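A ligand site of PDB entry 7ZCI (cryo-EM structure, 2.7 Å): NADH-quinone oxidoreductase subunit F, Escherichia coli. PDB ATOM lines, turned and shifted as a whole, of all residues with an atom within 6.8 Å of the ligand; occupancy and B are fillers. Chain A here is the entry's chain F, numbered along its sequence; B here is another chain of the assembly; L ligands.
SG of Cys 351 sits close to ND2 of Asn 196, at 3.3 Å.
SG of Cys 351 sits close to N of Trp 353.
OG of Ser 350 sits close to N of Gly 352.
The guanidinium group of Arg 358 lies close to the backbone carbonyl oxygen of Cys 354, 3.4 Å away.
A ring nitrogen (NE2) of His 400 is in hydrogen-bond range of the backbone carbonyl oxygen (O) of Phe 346, at 2.8 Å.
The backbone NH (N) of His 400 sits close to the side-chain sulfur (SG) of Cys 398 (3.4 Å).
OG1 of Thr 396 lies within hydrogen-bond range of O of Cys 398 (2.9 Å).
O of Thr 396 lies within hydrogen-bond range of NH2 of Arg 46 of chain B (3.4 Å).
CD1 of Ile 179 touches S1 of the ligand (3.7 Å).
Pro 197 touches the ligand (CG to S2, 3.5 Å).
Thr 396 touches the ligand (CB to S4, 3.8 Å).
Phe 397 touches the ligand.
His 400 touches the ligand.
N of Ala 401 touches S4 of the ligand (3.98 Å).
A sulfur (S3) of the ligand sits close to the side-chain hydroxyl of Ser 350, at 3.5 Å.
An iron atom (FE2) of the ligand is bound by the side-chain sulfur of Cys 357, 2.3 Å away.
N of Cys 354 lies close to S3 of the ligand, 3.2 Å away.
The side-chain sulfur (SG) of Cys 398 binds an iron atom (FE3) of the ligand, at 2.3 Å.
An iron atom (FE1) of the ligand is bound by the side-chain sulfur of Cys 354 (2.3 Å).
The side-chain sulfur (SG) of Cys 351 is bound to an iron atom (FE4) of the ligand.
N of Cys 351 sits close to S1 of the ligand, at 3.5 Å.
The backbone NH (N) of Trp 353 sits close to a sulfur (S3) of the ligand (3.3 Å).
N of Gly 352 lies close to S3 of the ligand.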
ATOM      1  N   ILE A 179     -27.994  12.987 -15.939  1.00  0.00           N
ATOM      2  CA  ILE A 179     -28.631  12.046 -16.862  1.00  0.00           C
ATOM      3  C   ILE A 179     -29.446  12.748 -17.938  1.00  0.00           C
ATOM      4  O   ILE A 179     -29.778  12.139 -18.950  1.00  0.00           O
ATOM      5  CB  ILE A 179     -29.478  11.047 -16.048  1.00  0.00           C
ATOM      6  CG1 ILE A 179     -29.823   9.791 -16.852  1.00  0.00           C
ATOM      7  CG2 ILE A 179     -30.718  11.714 -15.493  1.00  0.00           C
ATOM      8  CD1 ILE A 179     -28.681   9.192 -17.610  1.00  0.00           C
ATOM      9  N   GLU A 182     -28.046  12.441 -21.605  1.00  0.00           N
ATOM     10  CA  GLU A 182     -28.294  11.241 -22.396  1.00  0.00           C
ATOM     11  C   GLU A 182     -29.530  11.477 -23.251  1.00  0.00           C
ATOM     12  O   GLU A 182     -30.550  11.972 -22.757  1.00  0.00           O
ATOM     13  CB  GLU A 182     -28.477  10.030 -21.475  1.00  0.00           C
ATOM     14  CG  GLU A 182     -29.499   9.003 -21.924  1.00  0.00           C
ATOM     15  CD  GLU A 182     -28.946   8.005 -22.908  1.00  0.00           C
ATOM     16  OE1 GLU A 182     -27.748   8.086 -23.214  1.00  0.00           O
ATOM     17  OE2 GLU A 182     -29.706   7.144 -23.374  1.00  0.00           O
ATOM     18  N   ALA A 195     -36.261  12.288 -16.101  1.00  0.00           N
ATOM     19  CA  ALA A 195     -35.292  12.068 -17.174  1.00  0.00           C
ATOM     20  C   ALA A 195     -34.739  10.640 -17.155  1.00  0.00           C
ATOM     21  O   ALA A 195     -33.550  10.404 -17.042  1.00  0.00           O
ATOM     22  CB  ALA A 195     -34.173  13.097 -17.070  1.00  0.00           C
ATOM     23  N   ASN A 196     -35.636   9.692 -17.264  1.00  0.00           N
ATOM     24  CA  ASN A 196     -35.193   8.327 -17.479  1.00  0.00           C
ATOM     25  C   ASN A 196     -34.866   8.127 -18.949  1.00  0.00           C
ATOM     26  O   ASN A 196     -35.574   8.632 -19.817  1.00  0.00           O
ATOM     27  CB  ASN A 196     -36.266   7.328 -17.047  1.00  0.00           C
ATOM     28  CG  ASN A 196     -36.623   7.443 -15.587  1.00  0.00           C
ATOM     29  OD1 ASN A 196     -37.754   7.752 -15.248  1.00  0.00           O
ATOM     30  ND2 ASN A 196     -35.660   7.190 -14.727  1.00  0.00           N
ATOM     31  N   PRO A 197     -33.792   7.401 -19.272  1.00  0.00           N
ATOM     32  CA  PRO A 197     -33.530   7.071 -20.669  1.00  0.00           C
ATOM     33  C   PRO A 197     -34.516   6.029 -21.195  1.00  0.00           C
ATOM     34  O   PRO A 197     -35.322   5.463 -20.466  1.00  0.00           O
ATOM     35  CB  PRO A 197     -32.098   6.544 -20.645  1.00  0.00           C
ATOM     36  CG  PRO A 197     -31.830   6.217 -19.255  1.00  0.00           C
ATOM     37  CD  PRO A 197     -32.663   7.075 -18.400  1.00  0.00           C
ATOM     38  N   PHE A 346     -21.075   9.813  -9.699  1.00  0.00           N
ATOM     39  CA  PHE A 346     -21.784   8.900 -10.582  1.00  0.00           C
ATOM     40  C   PHE A 346     -22.939   8.205  -9.886  1.00  0.00           C
ATOM     41  O   PHE A 346     -23.980   7.977 -10.505  1.00  0.00           O
ATOM     42  CB  PHE A 346     -20.813   7.866 -11.150  1.00  0.00           C
ATOM     43  CG  PHE A 346     -20.028   8.361 -12.319  1.00  0.00           C
ATOM     44  CD1 PHE A 346     -20.664   8.883 -13.436  1.00  0.00           C
ATOM     45  CD2 PHE A 346     -18.647   8.330 -12.310  1.00  0.00           C
ATOM     46  CE1 PHE A 346     -19.943   9.344 -14.506  1.00  0.00           C
ATOM     47  CE2 PHE A 346     -17.926   8.791 -13.381  1.00  0.00           C
ATOM     48  CZ  PHE A 346     -18.574   9.300 -14.474  1.00  0.00           C
ATOM     49  N   GLU A 349     -25.737  10.738  -9.327  1.00  0.00           N
ATOM     50  CA  GLU A 349     -26.324  11.161 -10.580  1.00  0.00           C
ATOM     51  C   GLU A 349     -26.990  10.012 -11.323  1.00  0.00           C
ATOM     52  O   GLU A 349     -27.357  10.174 -12.487  1.00  0.00           O
ATOM     53  CB  GLU A 349     -25.285  11.844 -11.458  1.00  0.00           C
ATOM     54  CG  GLU A 349     -24.964  13.238 -10.985  1.00  0.00           C
ATOM     55  CD  GLU A 349     -26.198  14.110 -10.881  1.00  0.00           C
ATOM     56  OE1 GLU A 349     -26.991  14.132 -11.842  1.00  0.00           O
ATOM     57  OE2 GLU A 349     -26.377  14.764  -9.837  1.00  0.00           O
ATOM     58  N   SER A 350     -27.132   8.864 -10.675  1.00  0.00           N
ATOM     59  CA  SER A 350     -27.956   7.792 -11.202  1.00  0.00           C
ATOM     60  C   SER A 350     -29.398   8.281 -11.320  1.00  0.00           C
ATOM     61  O   SER A 350     -29.864   9.107 -10.543  1.00  0.00           O
ATOM     62  CB  SER A 350     -27.892   6.585 -10.273  1.00  0.00           C
ATOM     63  OG  SER A 350     -28.669   5.505 -10.731  1.00  0.00           O
ATOM     64  N   CYS A 351     -30.099   7.787 -12.340  1.00  0.00           N
ATOM     65  CA  CYS A 351     -31.490   8.170 -12.509  1.00  0.00           C
ATOM     66  C   CYS A 351     -32.431   7.233 -11.771  1.00  0.00           C
ATOM     67  O   CYS A 351     -33.625   7.525 -11.702  1.00  0.00           O
ATOM     68  CB  CYS A 351     -31.840   8.215 -13.993  1.00  0.00           C
ATOM     69  SG  CYS A 351     -32.396   6.671 -14.682  1.00  0.00           S
ATOM     70  N   GLY A 352     -31.916   6.158 -11.198  1.00  0.00           N
ATOM     71  CA  GLY A 352     -32.704   5.273 -10.380  1.00  0.00           C
ATOM     72  C   GLY A 352     -33.489   4.221 -11.117  1.00  0.00           C
ATOM     73  O   GLY A 352     -34.190   3.435 -10.476  1.00  0.00           O
ATOM     74  N   TRP A 353     -33.384   4.169 -12.447  1.00  0.00           N
ATOM     75  CA  TRP A 353     -34.223   3.253 -13.225  1.00  0.00           C
ATOM     76  C   TRP A 353     -33.808   1.808 -13.015  1.00  0.00           C
ATOM     77  O   TRP A 353     -34.620   0.976 -12.599  1.00  0.00           O
ATOM     78  CB  TRP A 353     -34.155   3.635 -14.708  1.00  0.00           C
ATOM     79  CG  TRP A 353     -34.918   2.743 -15.644  1.00  0.00           C
ATOM     80  CD1 TRP A 353     -34.397   1.933 -16.598  1.00  0.00           C
ATOM     81  CD2 TRP A 353     -36.334   2.590 -15.730  1.00  0.00           C
ATOM     82  NE1 TRP A 353     -35.393   1.285 -17.265  1.00  0.00           N
ATOM     83  CE2 TRP A 353     -36.595   1.677 -16.756  1.00  0.00           C
ATOM     84  CE3 TRP A 353     -37.419   3.144 -15.038  1.00  0.00           C
ATOM     85  CZ2 TRP A 353     -37.887   1.284 -17.110  1.00  0.00           C
ATOM     86  CZ3 TRP A 353     -38.693   2.761 -15.393  1.00  0.00           C
ATOM     87  CH2 TRP A 353     -38.913   1.839 -16.415  1.00  0.00           C
ATOM     88  N   CYS A 354     -32.540   1.485 -13.257  1.00  0.00           N
ATOM     89  CA  CYS A 354     -32.119   0.103 -13.324  1.00  0.00           C
ATOM     90  C   CYS A 354     -31.205  -0.271 -12.164  1.00  0.00           C
ATOM     91  O   CYS A 354     -30.404   0.544 -11.693  1.00  0.00           O
ATOM     92  CB  CYS A 354     -31.473  -0.212 -14.686  1.00  0.00           C
ATOM     93  SG  CYS A 354     -29.824   0.314 -15.028  1.00  0.00           S
ATOM     94  N   THR A 355     -31.349  -1.523 -11.717  1.00  0.00           N
ATOM     95  CA  THR A 355     -30.737  -2.008 -10.477  1.00  0.00           C
ATOM     96  C   THR A 355     -29.215  -1.872 -10.389  1.00  0.00           C
ATOM     97  O   THR A 355     -28.747  -1.363  -9.349  1.00  0.00           O
ATOM     98  CB  THR A 355     -31.151  -3.465 -10.232  1.00  0.00           C
ATOM     99  OG1 THR A 355     -32.564  -3.544 -10.058  1.00  0.00           O
ATOM    100  CG2 THR A 355     -30.460  -4.038  -9.004  1.00  0.00           C
ATOM    101  N   PRO A 356     -28.397  -2.310 -11.371  1.00  0.00           N
ATOM    102  CA  PRO A 356     -26.942  -2.327 -11.121  1.00  0.00           C
ATOM    103  C   PRO A 356     -26.337  -0.964 -10.858  1.00  0.00           C
ATOM    104  O   PRO A 356     -25.608  -0.825  -9.884  1.00  0.00           O
ATOM    105  CB  PRO A 356     -26.382  -2.949 -12.416  1.00  0.00           C
ATOM    106  CG  PRO A 356     -27.495  -3.679 -12.986  1.00  0.00           C
ATOM    107  CD  PRO A 356     -28.666  -2.824 -12.716  1.00  0.00           C
ATOM    108  N   CYS A 357     -26.668   0.047 -11.659  1.00  0.00           N
ATOM    109  CA  CYS A 357     -26.198   1.397 -11.392  1.00  0.00           C
ATOM    110  C   CYS A 357     -26.729   1.904 -10.053  1.00  0.00           C
ATOM    111  O   CYS A 357     -25.937   2.144  -9.123  1.00  0.00           O
ATOM    112  CB  CYS A 357     -26.624   2.279 -12.550  1.00  0.00           C
ATOM    113  SG  CYS A 357     -26.642   4.053 -12.394  1.00  0.00           S
ATOM    114  N   ARG A 358     -28.052   1.905  -9.893  1.00  0.00           N
ATOM    115  CA  ARG A 358     -28.731   2.472  -8.717  1.00  0.00           C
ATOM    116  C   ARG A 358     -28.273   1.849  -7.399  1.00  0.00           C
ATOM    117  O   ARG A 358     -28.154   2.550  -6.397  1.00  0.00           O
ATOM    118  CB  ARG A 358     -30.245   2.297  -8.867  1.00  0.00           C
ATOM    119  CG  ARG A 358     -31.042   2.372  -7.554  1.00  0.00           C
ATOM    120  CD  ARG A 358     -32.530   2.207  -7.725  1.00  0.00           C
ATOM    121  NE  ARG A 358     -32.872   0.796  -7.675  1.00  0.00           N
ATOM    122  CZ  ARG A 358     -33.227   0.083  -8.733  1.00  0.00           C
ATOM    123  NH1 ARG A 358     -33.335   0.639  -9.934  1.00  0.00           N
ATOM    124  NH2 ARG A 358     -33.456  -1.212  -8.593  1.00  0.00           N
ATOM    125  N   LEU A 361     -23.450   1.147  -7.715  1.00  0.00           N
ATOM    126  CA  LEU A 361     -22.598   2.325  -7.569  1.00  0.00           C
ATOM    127  C   LEU A 361     -22.522   2.840  -6.135  1.00  0.00           C
ATOM    128  O   LEU A 361     -21.411   3.210  -5.716  1.00  0.00           O
ATOM    129  CB  LEU A 361     -23.057   3.417  -8.548  1.00  0.00           C
ATOM    130  CG  LEU A 361     -22.631   3.213  -9.999  1.00  0.00           C
ATOM    131  CD1 LEU A 361     -22.984   4.427 -10.817  1.00  0.00           C
ATOM    132  CD2 LEU A 361     -21.144   2.922 -10.088  1.00  0.00           C
ATOM    133  N   THR A 396     -26.472  -2.639 -17.967  1.00  0.00           N
ATOM    134  CA  THR A 396     -27.355  -1.603 -17.455  1.00  0.00           C
ATOM    135  C   THR A 396     -28.169  -1.005 -18.586  1.00  0.00           C
ATOM    136  O   THR A 396     -27.862  -1.187 -19.771  1.00  0.00           O
ATOM    137  CB  THR A 396     -26.559  -0.513 -16.738  1.00  0.00           C
ATOM    138  OG1 THR A 396     -25.584   0.024 -17.633  1.00  0.00           O
ATOM    139  CG2 THR A 396     -25.858  -1.089 -15.539  1.00  0.00           C
ATOM    140  N   PHE A 397     -29.234  -0.303 -18.204  1.00  0.00           N
ATOM    141  CA  PHE A 397     -30.202   0.186 -19.170  1.00  0.00           C
ATOM    142  C   PHE A 397     -29.604   1.243 -20.102  1.00  0.00           C
ATOM    143  O   PHE A 397     -29.833   1.196 -21.312  1.00  0.00           O
ATOM    144  CB  PHE A 397     -31.436   0.737 -18.448  1.00  0.00           C
ATOM    145  CG  PHE A 397     -32.585   1.016 -19.350  1.00  0.00           C
ATOM    146  CD1 PHE A 397     -33.411   0.000 -19.778  1.00  0.00           C
ATOM    147  CD2 PHE A 397     -32.827   2.299 -19.793  1.00  0.00           C
ATOM    148  CE1 PHE A 397     -34.465   0.251 -20.613  1.00  0.00           C
ATOM    149  CE2 PHE A 397     -33.888   2.561 -20.621  1.00  0.00           C
ATOM    150  CZ  PHE A 397     -34.704   1.534 -21.025  1.00  0.00           C
ATOM    151  N   CYS A 398     -28.818   2.168 -19.569  1.00  0.00           N
ATOM    152  CA  CYS A 398     -28.139   3.150 -20.401  1.00  0.00           C
ATOM    153  C   CYS A 398     -26.639   3.085 -20.124  1.00  0.00           C
ATOM    154  O   CYS A 398     -26.153   2.207 -19.420  1.00  0.00           O
ATOM    155  CB  CYS A 398     -28.734   4.535 -20.161  1.00  0.00           C
ATOM    156  SG  CYS A 398     -27.992   5.500 -18.842  1.00  0.00           S
ATOM    157  N   ALA A 399     -25.906   4.038 -20.695  1.00  0.00           N
ATOM    158  CA  ALA A 399     -24.449   4.017 -20.693  1.00  0.00           C
ATOM    159  C   ALA A 399     -23.837   4.805 -19.543  1.00  0.00           C
ATOM    160  O   ALA A 399     -22.620   4.999 -19.535  1.00  0.00           O
ATOM    161  CB  ALA A 399     -23.922   4.539 -22.024  1.00  0.00           C
ATOM    162  N   HIS A 400     -24.642   5.256 -18.584  1.00  0.00           N
ATOM    163  CA  HIS A 400     -24.115   6.007 -17.451  1.00  0.00           C
ATOM    164  C   HIS A 400     -23.210   5.148 -16.584  1.00  0.00           C
ATOM    165  O   HIS A 400     -22.112   5.569 -16.212  1.00  0.00           O
ATOM    166  CB  HIS A 400     -25.288   6.569 -16.633  1.00  0.00           C
ATOM    167  CG  HIS A 400     -24.906   7.039 -15.267  1.00  0.00           C
ATOM    168  ND1 HIS A 400     -24.491   8.326 -15.007  1.00  0.00           N
ATOM    169  CD2 HIS A 400     -24.894   6.391 -14.079  1.00  0.00           C
ATOM    170  CE1 HIS A 400     -24.233   8.453 -13.723  1.00  0.00           C
ATOM    171  NE2 HIS A 400     -24.472   7.298 -13.132  1.00  0.00           N
ATOM    172  N   ALA A 401     -23.636   3.931 -16.261  1.00  0.00           N
ATOM    173  CA  ALA A 401     -22.868   3.045 -15.388  1.00  0.00           C
ATOM    174  C   ALA A 401     -21.586   2.472 -16.007  1.00  0.00           C
ATOM    175  O   ALA A 401     -20.607   2.326 -15.269  1.00  0.00           O
ATOM    176  CB  ALA A 401     -23.767   1.911 -14.885  1.00  0.00           C
ATOM    177  N   PRO A 402     -21.536   2.097 -17.304  1.00  0.00           N
ATOM    178  CA  PRO A 402     -20.215   1.752 -17.869  1.00  0.00           C
ATOM    179  C   PRO A 402     -19.219   2.892 -17.826  1.00  0.00           C
ATOM    180  O   PRO A 402     -18.037   2.676 -17.521  1.00  0.00           O
ATOM    181  CB  PRO A 402     -20.546   1.343 -19.300  1.00  0.00           C
ATOM    182  CG  PRO A 402     -21.896   0.861 -19.238  1.00  0.00           C
ATOM    183  CD  PRO A 402     -22.598   1.701 -18.243  1.00  0.00           C
ATOM    184  N   ALA B  44     -36.155  -2.790 -16.629  1.00  0.00           N
ATOM    185  CA  ALA B  44     -35.718  -2.007 -15.481  1.00  0.00           C
ATOM    186  C   ALA B  44     -34.849  -2.813 -14.528  1.00  0.00           C
ATOM    187  O   ALA B  44     -33.688  -2.480 -14.324  1.00  0.00           O
ATOM    188  CB  ALA B  44     -36.920  -1.426 -14.733  1.00  0.00           C
ATOM    189  N   ARG B  46     -33.201  -5.495 -14.478  1.00  0.00           N
ATOM    190  CA  ARG B  46     -31.996  -6.141 -15.010  1.00  0.00           C
ATOM    191  C   ARG B  46     -31.787  -7.542 -14.443  1.00  0.00           C
ATOM    192  O   ARG B  46     -30.663  -8.047 -14.416  1.00  0.00           O
ATOM    193  CB  ARG B  46     -30.730  -5.300 -14.833  1.00  0.00           C
ATOM    194  CG  ARG B  46     -30.870  -3.855 -15.251  1.00  0.00           C
ATOM    195  CD  ARG B  46     -31.373  -3.680 -16.637  1.00  0.00           C
ATOM    196  NE  ARG B  46     -30.376  -3.972 -17.646  1.00  0.00           N
ATOM    197  CZ  ARG B  46     -30.558  -3.768 -18.943  1.00  0.00           C
ATOM    198  NH1 ARG B  46     -31.681  -3.256 -19.407  1.00  0.00           N
ATOM    199  NH2 ARG B  46     -29.598  -4.109 -19.796  1.00  0.00           N
ATOM    200  N   HIS B 176     -31.641   8.893  -7.530  1.00  0.00           N
ATOM    201  CA  HIS B 176     -30.657   7.839  -7.727  1.00  0.00           C
ATOM    202  C   HIS B 176     -30.844   6.530  -6.987  1.00  0.00           C
ATOM    203  O   HIS B 176     -30.972   5.483  -7.624  1.00  0.00           O
ATOM    204  CB  HIS B 176     -29.321   8.455  -7.307  1.00  0.00           C
ATOM    205  CG  HIS B 176     -29.479   9.447  -6.188  1.00  0.00           C
ATOM    206  ND1 HIS B 176     -29.539   9.065  -4.871  1.00  0.00           N
ATOM    207  CD2 HIS B 176     -29.657  10.787  -6.206  1.00  0.00           C
ATOM    208  CE1 HIS B 176     -29.712  10.138  -4.118  1.00  0.00           C
ATOM    209  NE2 HIS B 176     -29.788  11.197  -4.904  1.00  0.00           N
HETATM  210 FE1  LIG L   1     -29.670   2.626 -15.246  1.00  0.00          FE
HETATM  211 FE2  LIG L   1     -28.153   4.386 -14.118  1.00  0.00          FE
HETATM  212 FE3  LIG L   1     -28.718   4.728 -16.771  1.00  0.00          FE
HETATM  213 FE4  LIG L   1     -30.585   5.229 -14.960  1.00  0.00          FE
HETATM  214  S1  LIG L   1     -28.607   6.387 -15.170  1.00  0.00           S
HETATM  215  S2  LIG L   1     -30.854   3.864 -16.789  1.00  0.00           S
HETATM  216  S3  LIG L   1     -30.189   3.700 -13.293  1.00  0.00           S
HETATM  217  S4  LIG L   1     -27.489   3.019 -15.855  1.00  0.00           S
